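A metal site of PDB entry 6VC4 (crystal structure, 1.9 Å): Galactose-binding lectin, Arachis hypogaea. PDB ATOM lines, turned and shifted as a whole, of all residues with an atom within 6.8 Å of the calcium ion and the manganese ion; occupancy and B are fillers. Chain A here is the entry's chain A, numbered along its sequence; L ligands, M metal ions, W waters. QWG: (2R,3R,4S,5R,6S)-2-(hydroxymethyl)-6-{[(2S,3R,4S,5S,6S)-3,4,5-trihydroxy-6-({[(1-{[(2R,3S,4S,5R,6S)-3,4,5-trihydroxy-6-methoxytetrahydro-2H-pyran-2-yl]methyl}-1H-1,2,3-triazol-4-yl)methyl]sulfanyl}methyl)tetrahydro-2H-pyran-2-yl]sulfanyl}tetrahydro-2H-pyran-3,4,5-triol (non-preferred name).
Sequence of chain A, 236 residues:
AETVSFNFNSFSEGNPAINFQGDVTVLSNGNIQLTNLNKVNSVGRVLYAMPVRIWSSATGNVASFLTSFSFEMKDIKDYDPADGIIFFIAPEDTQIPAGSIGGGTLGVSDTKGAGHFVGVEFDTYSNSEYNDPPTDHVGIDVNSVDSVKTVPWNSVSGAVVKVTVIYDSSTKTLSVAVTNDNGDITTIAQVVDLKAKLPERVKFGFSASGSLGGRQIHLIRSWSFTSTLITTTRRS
An oxygen (O3) of the ligand sits at hydrogen-bond distance from the side-chain carboxylate of Asp 83 (2.6 Å).
The backbone NH (N) of Gly 104 sits at hydrogen-bond distance from an oxygen (O3) of the ligand (3.0 Å).
The side-chain amide nitrogen of Asn 127 lies within hydrogen-bond range of an oxygen (O3) of the ligand, at 3.2 Å.
O of Glu 121 lies within hydrogen-bond range of N of Gly 139.
Of the 24 residues printed, 4 come within 4 Å of the calcium ion.
The calcium ion is bound by water W4, O of Tyr 125, OD2 of Asp 132, water W1, OD2 of Asp 123, OD1 of Asn 127 and OD1 of Asp 123.
The manganese ion is bound by a ring nitrogen (NE2) of His 137 (2.1 Å), the side-chain carboxylate of Asp 123 (2.1 Å), water W2 (2.2 Å), the side-chain carboxylate of Glu 121 (2.3 Å), the side-chain carboxylate of Asp 132 (2.3 Å) and water W3 (2.5 Å).
The manganese ion has six donor atoms within binding distance.
Water W3 bridges the backbone carbonyl oxygen (O) of Val 145 (2.6 Å) and the side-chain carboxylate (OE1) of Glu 121 (2.6 Å).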
ATOM      1  N   ASP A  83     -23.944  17.459   5.714  1.00  0.00           N
ATOM      2  CA  ASP A  83     -23.421  18.697   5.120  1.00  0.00           C
ATOM      3  C   ASP A  83     -21.914  18.954   5.291  1.00  0.00           C
ATOM      4  O   ASP A  83     -21.360  19.791   4.585  1.00  0.00           O
ATOM      5  CB  ASP A  83     -24.178  19.879   5.688  1.00  0.00           C
ATOM      6  CG  ASP A  83     -25.453  20.082   4.926  1.00  0.00           C
ATOM      7  OD1 ASP A  83     -26.500  19.465   5.318  1.00  0.00           O
ATOM      8  OD2 ASP A  83     -25.416  20.834   3.939  1.00  0.00           O
ATOM      9  N   GLY A 103     -28.179  21.763   8.287  1.00  0.00           N
ATOM     10  CA  GLY A 103     -27.794  21.945   6.890  1.00  0.00           C
ATOM     11  C   GLY A 103     -26.439  22.634   6.702  1.00  0.00           C
ATOM     12  O   GLY A 103     -25.431  22.234   7.304  1.00  0.00           O
ATOM     13  N   GLY A 104     -26.458  23.697   5.905  1.00  0.00           N
ATOM     14  CA  GLY A 104     -25.299  24.515   5.531  1.00  0.00           C
ATOM     15  C   GLY A 104     -24.695  25.361   6.638  1.00  0.00           C
ATOM     16  O   GLY A 104     -23.612  25.927   6.458  1.00  0.00           O
ATOM     17  N   THR A 105     -25.439  25.533   7.758  1.00  0.00           N
ATOM     18  CA  THR A 105     -25.010  26.320   8.927  1.00  0.00           C
ATOM     19  C   THR A 105     -23.899  25.584   9.689  1.00  0.00           C
ATOM     20  O   THR A 105     -23.269  26.188  10.551  1.00  0.00           O
ATOM     21  CB  THR A 105     -26.222  26.632   9.873  1.00  0.00           C
ATOM     22  OG1 THR A 105     -26.597  25.475  10.653  1.00  0.00           O
ATOM     23  CG2 THR A 105     -27.405  27.226   9.130  1.00  0.00           C
ATOM     24  N   LEU A 106     -23.765  24.259   9.438  1.00  0.00           N
ATOM     25  CA  LEU A 106     -22.798  23.316  10.014  1.00  0.00           C
ATOM     26  C   LEU A 106     -22.883  23.276  11.558  1.00  0.00           C
ATOM     27  O   LEU A 106     -21.943  22.809  12.229  1.00  0.00           O
ATOM     28  CB  LEU A 106     -21.354  23.622   9.543  1.00  0.00           C
ATOM     29  CG  LEU A 106     -21.092  23.578   8.031  1.00  0.00           C
ATOM     30  CD1 LEU A 106     -19.649  24.075   7.729  1.00  0.00           C
ATOM     31  CD2 LEU A 106     -21.341  22.170   7.440  1.00  0.00           C
ATOM     32  N   GLU A 121     -13.714  24.327   8.039  1.00  0.00           N
ATOM     33  CA  GLU A 121     -14.813  23.470   7.588  1.00  0.00           C
ATOM     34  C   GLU A 121     -14.375  22.542   6.453  1.00  0.00           C
ATOM     35  O   GLU A 121     -13.544  22.894   5.596  1.00  0.00           O
ATOM     36  CB  GLU A 121     -16.016  24.308   7.144  1.00  0.00           C
ATOM     37  CG  GLU A 121     -15.662  25.300   6.049  1.00  0.00           C
ATOM     38  CD  GLU A 121     -16.836  25.805   5.245  1.00  0.00           C
ATOM     39  OE1 GLU A 121     -17.673  26.512   5.827  1.00  0.00           O
ATOM     40  OE2 GLU A 121     -16.869  25.554   4.020  1.00  0.00           O
ATOM     41  N   PHE A 122     -14.935  21.335   6.488  1.00  0.00           N
ATOM     42  CA  PHE A 122     -14.792  20.230   5.533  1.00  0.00           C
ATOM     43  C   PHE A 122     -16.209  20.043   4.949  1.00  0.00           C
ATOM     44  O   PHE A 122     -16.983  19.207   5.395  1.00  0.00           O
ATOM     45  CB  PHE A 122     -14.219  18.985   6.265  1.00  0.00           C
ATOM     46  CG  PHE A 122     -12.898  19.297   6.923  1.00  0.00           C
ATOM     47  CD1 PHE A 122     -11.707  19.167   6.225  1.00  0.00           C
ATOM     48  CD2 PHE A 122     -12.854  19.776   8.228  1.00  0.00           C
ATOM     49  CE1 PHE A 122     -10.490  19.505   6.826  1.00  0.00           C
ATOM     50  CE2 PHE A 122     -11.625  20.125   8.821  1.00  0.00           C
ATOM     51  CZ  PHE A 122     -10.464  19.998   8.107  1.00  0.00           C
ATOM     52  N   ASP A 123     -16.545  20.928   4.020  1.00  0.00           N
ATOM     53  CA  ASP A 123     -17.858  21.119   3.442  1.00  0.00           C
ATOM     54  C   ASP A 123     -18.161  20.250   2.226  1.00  0.00           C
ATOM     55  O   ASP A 123     -17.550  20.425   1.174  1.00  0.00           O
ATOM     56  CB  ASP A 123     -17.980  22.600   3.079  1.00  0.00           C
ATOM     57  CG  ASP A 123     -19.414  23.022   2.841  1.00  0.00           C
ATOM     58  OD1 ASP A 123     -20.287  22.136   2.770  1.00  0.00           O
ATOM     59  OD2 ASP A 123     -19.666  24.225   2.810  1.00  0.00           O
ATOM     60  N   THR A 124     -19.216  19.382   2.336  1.00  0.00           N
ATOM     61  CA  THR A 124     -19.590  18.424   1.290  1.00  0.00           C
ATOM     62  C   THR A 124     -20.877  18.753   0.515  1.00  0.00           C
ATOM     63  O   THR A 124     -21.385  17.884  -0.214  1.00  0.00           O
ATOM     64  CB  THR A 124     -19.694  17.025   1.908  1.00  0.00           C
ATOM     65  OG1 THR A 124     -20.919  16.896   2.640  1.00  0.00           O
ATOM     66  CG2 THR A 124     -18.495  16.686   2.789  1.00  0.00           C
ATOM     67  N   TYR A 125     -21.355  19.998   0.590  1.00  0.00           N
ATOM     68  CA  TYR A 125     -22.583  20.415  -0.127  1.00  0.00           C
ATOM     69  C   TYR A 125     -22.507  21.902  -0.430  1.00  0.00           C
ATOM     70  O   TYR A 125     -22.248  22.701   0.476  1.00  0.00           O
ATOM     71  CB  TYR A 125     -23.882  20.060   0.649  1.00  0.00           C
ATOM     72  CG  TYR A 125     -25.126  20.460  -0.131  1.00  0.00           C
ATOM     73  CD1 TYR A 125     -25.691  19.597  -1.064  1.00  0.00           C
ATOM     74  CD2 TYR A 125     -25.648  21.749  -0.035  1.00  0.00           C
ATOM     75  CE1 TYR A 125     -26.755  19.998  -1.863  1.00  0.00           C
ATOM     76  CE2 TYR A 125     -26.663  22.182  -0.873  1.00  0.00           C
ATOM     77  CZ  TYR A 125     -27.249  21.290  -1.759  1.00  0.00           C
ATOM     78  OH  TYR A 125     -28.305  21.685  -2.538  1.00  0.00           O
ATOM     79  N   SER A 126     -22.758  22.261  -1.693  1.00  0.00           N
ATOM     80  CA  SER A 126     -22.679  23.637  -2.166  1.00  0.00           C
ATOM     81  C   SER A 126     -23.974  24.441  -1.890  1.00  0.00           C
ATOM     82  O   SER A 126     -24.955  24.318  -2.624  1.00  0.00           O
ATOM     83  CB  SER A 126     -22.322  23.666  -3.656  1.00  0.00           C
ATOM     84  OG  SER A 126     -22.078  24.991  -4.094  1.00  0.00           O
ATOM     85  N   ASN A 127     -23.943  25.264  -0.828  1.00  0.00           N
ATOM     86  CA  ASN A 127     -25.004  26.183  -0.425  1.00  0.00           C
ATOM     87  C   ASN A 127     -24.811  27.544  -1.097  1.00  0.00           C
ATOM     88  O   ASN A 127     -24.007  28.343  -0.632  1.00  0.00           O
ATOM     89  CB  ASN A 127     -25.044  26.343   1.100  1.00  0.00           C
ATOM     90  CG  ASN A 127     -25.412  25.100   1.835  1.00  0.00           C
ATOM     91  OD1 ASN A 127     -24.548  24.301   2.213  1.00  0.00           O
ATOM     92  ND2 ASN A 127     -26.696  24.912   2.086  1.00  0.00           N
ATOM     93  N   TYR A 130     -24.754  30.702   1.003  1.00  0.00           N
ATOM     94  CA  TYR A 130     -23.542  31.022   1.762  1.00  0.00           C
ATOM     95  C   TYR A 130     -22.337  31.201   0.826  1.00  0.00           C
ATOM     96  O   TYR A 130     -21.196  31.174   1.266  1.00  0.00           O
ATOM     97  CB  TYR A 130     -23.269  29.961   2.839  1.00  0.00           C
ATOM     98  CG  TYR A 130     -24.461  29.704   3.735  1.00  0.00           C
ATOM     99  CD1 TYR A 130     -25.152  30.752   4.334  1.00  0.00           C
ATOM    100  CD2 TYR A 130     -24.869  28.406   4.026  1.00  0.00           C
ATOM    101  CE1 TYR A 130     -26.263  30.525   5.141  1.00  0.00           C
ATOM    102  CE2 TYR A 130     -25.979  28.155   4.827  1.00  0.00           C
ATOM    103  CZ  TYR A 130     -26.661  29.223   5.387  1.00  0.00           C
ATOM    104  OH  TYR A 130     -27.733  28.989   6.206  1.00  0.00           O
ATOM    105  N   ASN A 131     -22.618  31.408  -0.488  1.00  0.00           N
ATOM    106  CA  ASN A 131     -21.649  31.609  -1.571  1.00  0.00           C
ATOM    107  C   ASN A 131     -20.595  30.487  -1.612  1.00  0.00           C
ATOM    108  O   ASN A 131     -19.423  30.746  -1.855  1.00  0.00           O
ATOM    109  CB  ASN A 131     -20.984  33.004  -1.479  1.00  0.00           C
ATOM    110  CG  ASN A 131     -21.940  34.141  -1.753  1.00  0.00           C
ATOM    111  OD1 ASN A 131     -22.579  34.221  -2.817  1.00  0.00           O
ATOM    112  ND2 ASN A 131     -22.071  35.054  -0.787  1.00  0.00           N
ATOM    113  N   ASP A 132     -21.039  29.237  -1.377  1.00  0.00           N
ATOM    114  CA  ASP A 132     -20.163  28.067  -1.412  1.00  0.00           C
ATOM    115  C   ASP A 132     -19.566  27.862  -2.812  1.00  0.00           C
ATOM    116  O   ASP A 132     -20.313  28.014  -3.790  1.00  0.00           O
ATOM    117  CB  ASP A 132     -20.936  26.810  -1.035  1.00  0.00           C
ATOM    118  CG  ASP A 132     -20.910  26.440   0.435  1.00  0.00           C
ATOM    119  OD1 ASP A 132     -20.018  26.920   1.155  1.00  0.00           O
ATOM    120  OD2 ASP A 132     -21.739  25.595   0.848  1.00  0.00           O
ATOM    121  N   PRO A 133     -18.304  27.417  -2.930  1.00  0.00           N
ATOM    122  CA  PRO A 133     -17.778  27.084  -4.272  1.00  0.00           C
ATOM    123  C   PRO A 133     -18.547  25.874  -4.858  1.00  0.00           C
ATOM    124  O   PRO A 133     -19.271  25.206  -4.089  1.00  0.00           O
ATOM    125  CB  PRO A 133     -16.280  26.805  -4.025  1.00  0.00           C
ATOM    126  CG  PRO A 133     -16.156  26.526  -2.584  1.00  0.00           C
ATOM    127  CD  PRO A 133     -17.292  27.181  -1.865  1.00  0.00           C
ATOM    128  N   HIS A 137     -15.098  21.243  -0.437  1.00  0.00           N
ATOM    129  CA  HIS A 137     -14.015  22.177  -0.131  1.00  0.00           C
ATOM    130  C   HIS A 137     -13.678  22.286   1.336  1.00  0.00           C
ATOM    131  O   HIS A 137     -14.493  22.016   2.217  1.00  0.00           O
ATOM    132  CB  HIS A 137     -14.378  23.588  -0.661  1.00  0.00           C
ATOM    133  CG  HIS A 137     -15.681  24.106  -0.130  1.00  0.00           C
ATOM    134  ND1 HIS A 137     -16.915  23.655  -0.622  1.00  0.00           N
ATOM    135  CD2 HIS A 137     -15.911  25.002   0.861  1.00  0.00           C
ATOM    136  CE1 HIS A 137     -17.836  24.318   0.051  1.00  0.00           C
ATOM    137  NE2 HIS A 137     -17.288  25.122   0.966  1.00  0.00           N
ATOM    138  N   VAL A 138     -12.452  22.753   1.579  1.00  0.00           N
ATOM    139  CA  VAL A 138     -11.976  23.076   2.909  1.00  0.00           C
ATOM    140  C   VAL A 138     -12.043  24.589   2.967  1.00  0.00           C
ATOM    141  O   VAL A 138     -11.646  25.245   2.008  1.00  0.00           O
ATOM    142  CB  VAL A 138     -10.586  22.489   3.235  1.00  0.00           C
ATOM    143  CG1 VAL A 138     -10.175  22.847   4.663  1.00  0.00           C
ATOM    144  CG2 VAL A 138     -10.554  20.977   3.042  1.00  0.00           C
ATOM    145  N   GLY A 139     -12.621  25.116   4.021  1.00  0.00           N
ATOM    146  CA  GLY A 139     -12.761  26.553   4.167  1.00  0.00           C
ATOM    147  C   GLY A 139     -12.252  27.046   5.496  1.00  0.00           C
ATOM    148  O   GLY A 139     -12.209  26.279   6.464  1.00  0.00           O
ATOM    149  N   ASP A 141     -13.183  29.916   8.138  1.00  0.00           N
ATOM    150  CA  ASP A 141     -14.399  30.676   8.503  1.00  0.00           C
ATOM    151  C   ASP A 141     -14.175  31.610   9.659  1.00  0.00           C
ATOM    152  O   ASP A 141     -13.630  31.209  10.681  1.00  0.00           O
ATOM    153  CB  ASP A 141     -15.519  29.698   8.894  1.00  0.00           C
ATOM    154  CG  ASP A 141     -16.046  28.844   7.761  1.00  0.00           C
ATOM    155  OD1 ASP A 141     -15.614  29.049   6.594  1.00  0.00           O
ATOM    156  OD2 ASP A 141     -16.920  27.985   8.029  1.00  0.00           O
ATOM    157  N   VAL A 145     -20.307  31.129   7.776  1.00  0.00           N
ATOM    158  CA  VAL A 145     -20.144  29.933   6.939  1.00  0.00           C
ATOM    159  C   VAL A 145     -19.961  30.390   5.475  1.00  0.00           C
ATOM    160  O   VAL A 145     -19.742  29.566   4.599  1.00  0.00           O
ATOM    161  CB  VAL A 145     -21.193  28.798   7.118  1.00  0.00           C
ATOM    162  CG1 VAL A 145     -20.949  28.012   8.414  1.00  0.00           C
ATOM    163  CG2 VAL A 145     -22.622  29.309   7.055  1.00  0.00           C
ATOM    164  N   ASP A 146     -19.966  31.735   5.222  1.00  0.00           N
ATOM    165  CA  ASP A 146     -19.536  32.335   3.957  1.00  0.00           C
ATOM    166  C   ASP A 146     -18.025  32.551   4.186  1.00  0.00           C
ATOM    167  O   ASP A 146     -17.616  33.567   4.771  1.00  0.00           O
ATOM    168  CB  ASP A 146     -20.311  33.625   3.617  1.00  0.00           C
ATOM    169  CG  ASP A 146     -20.010  34.236   2.237  1.00  0.00           C
ATOM    170  OD1 ASP A 146     -18.972  33.869   1.620  1.00  0.00           O
ATOM    171  OD2 ASP A 146     -20.793  35.113   1.783  1.00  0.00           O
ATOM    172  N   SER A 147     -17.234  31.523   3.854  1.00  0.00           N
ATOM    173  CA  SER A 147     -15.807  31.408   4.110  1.00  0.00           C
ATOM    174  C   SER A 147     -14.993  32.594   3.611  1.00  0.00           C
ATOM    175  O   SER A 147     -15.214  33.099   2.513  1.00  0.00           O
ATOM    176  CB  SER A 147     -15.242  30.137   3.478  1.00  0.00           C
ATOM    177  OG  SER A 147     -15.885  28.975   3.953  1.00  0.00           O
ATOM    178  N   THR A 150     -11.504  29.434   0.596  1.00  0.00           N
ATOM    179  CA  THR A 150     -11.733  28.014   0.386  1.00  0.00           C
ATOM    180  C   THR A 150     -10.690  27.449  -0.566  1.00  0.00           C
ATOM    181  O   THR A 150     -10.070  28.186  -1.331  1.00  0.00           O
ATOM    182  CB  THR A 150     -13.166  27.671  -0.151  1.00  0.00           C
ATOM    183  OG1 THR A 150     -13.337  28.219  -1.451  1.00  0.00           O
ATOM    184  CG2 THR A 150     -14.254  28.126   0.762  1.00  0.00           C
HETATM  185  C4  QWG L   1     -28.149  20.331   2.151  1.00  0.00           C
HETATM  186  C3  QWG L   1     -28.354  21.821   2.410  1.00  0.00           C
HETATM  187  C5  QWG L   1     -29.120  19.867   1.068  1.00  0.00           C
HETATM  188  C1  QWG L   1     -30.749  21.515   1.633  1.00  0.00           C
HETATM  189  C2  QWG L   1     -29.815  22.135   2.682  1.00  0.00           C
HETATM  190  C6  QWG L   1     -29.023  18.389   0.754  1.00  0.00           C
HETATM  191  C10 QWG L   1     -35.712  22.249  -1.079  1.00  0.00           C
HETATM  192  C9  QWG L   1     -35.641  20.923  -0.353  1.00  0.00           C
HETATM  193  C11 QWG L   1     -34.320  22.870  -1.265  1.00  0.00           C
HETATM  194  C7  QWG L   1     -33.479  21.535   0.616  1.00  0.00           C
HETATM  195  C8  QWG L   1     -34.911  21.112   0.961  1.00  0.00           C
HETATM  196  O5  QWG L   1     -30.468  20.126   1.477  1.00  0.00           O
HETATM  197  O2  QWG L   1     -30.031  23.536   2.752  1.00  0.00           O
HETATM  198  O3  QWG L   1     -27.571  22.244   3.520  1.00  0.00           O
HETATM  199  O4  QWG L   1     -28.327  19.583   3.361  1.00  0.00           O
HETATM  200  O6  QWG L   1     -29.512  18.060  -0.551  1.00  0.00           O
HETATM  201  O11 QWG L   1     -33.494  22.781  -0.086  1.00  0.00           O
HETATM  202  O8  QWG L   1     -34.943  19.933   1.756  1.00  0.00           O
HETATM  203  O9  QWG L   1     -36.956  20.425  -0.098  1.00  0.00           O
HETATM  204  O10 QWG L   1     -36.367  22.056  -2.337  1.00  0.00           O
HETATM  205  S1  QWG L   1     -32.472  21.732   2.116  1.00  0.00           S
HETATM  206 CA    CA M   1     -22.085  23.858   2.385  1.00  0.00          CA
HETATM  207 MN    MN M   2     -18.456  25.916   2.453  1.00  0.00          MN
HETATM  208  O   HOH W   1     -22.192  25.492   4.239  1.00  0.00           O
HETATM  209  O   HOH W   2     -17.346  27.800   1.963  1.00  0.00           O
HETATM  210  O   HOH W   3     -19.767  26.980   4.304  1.00  0.00           O
HETATM  211  O   HOH W   4     -22.863  22.123   3.545  1.00  0.00           O
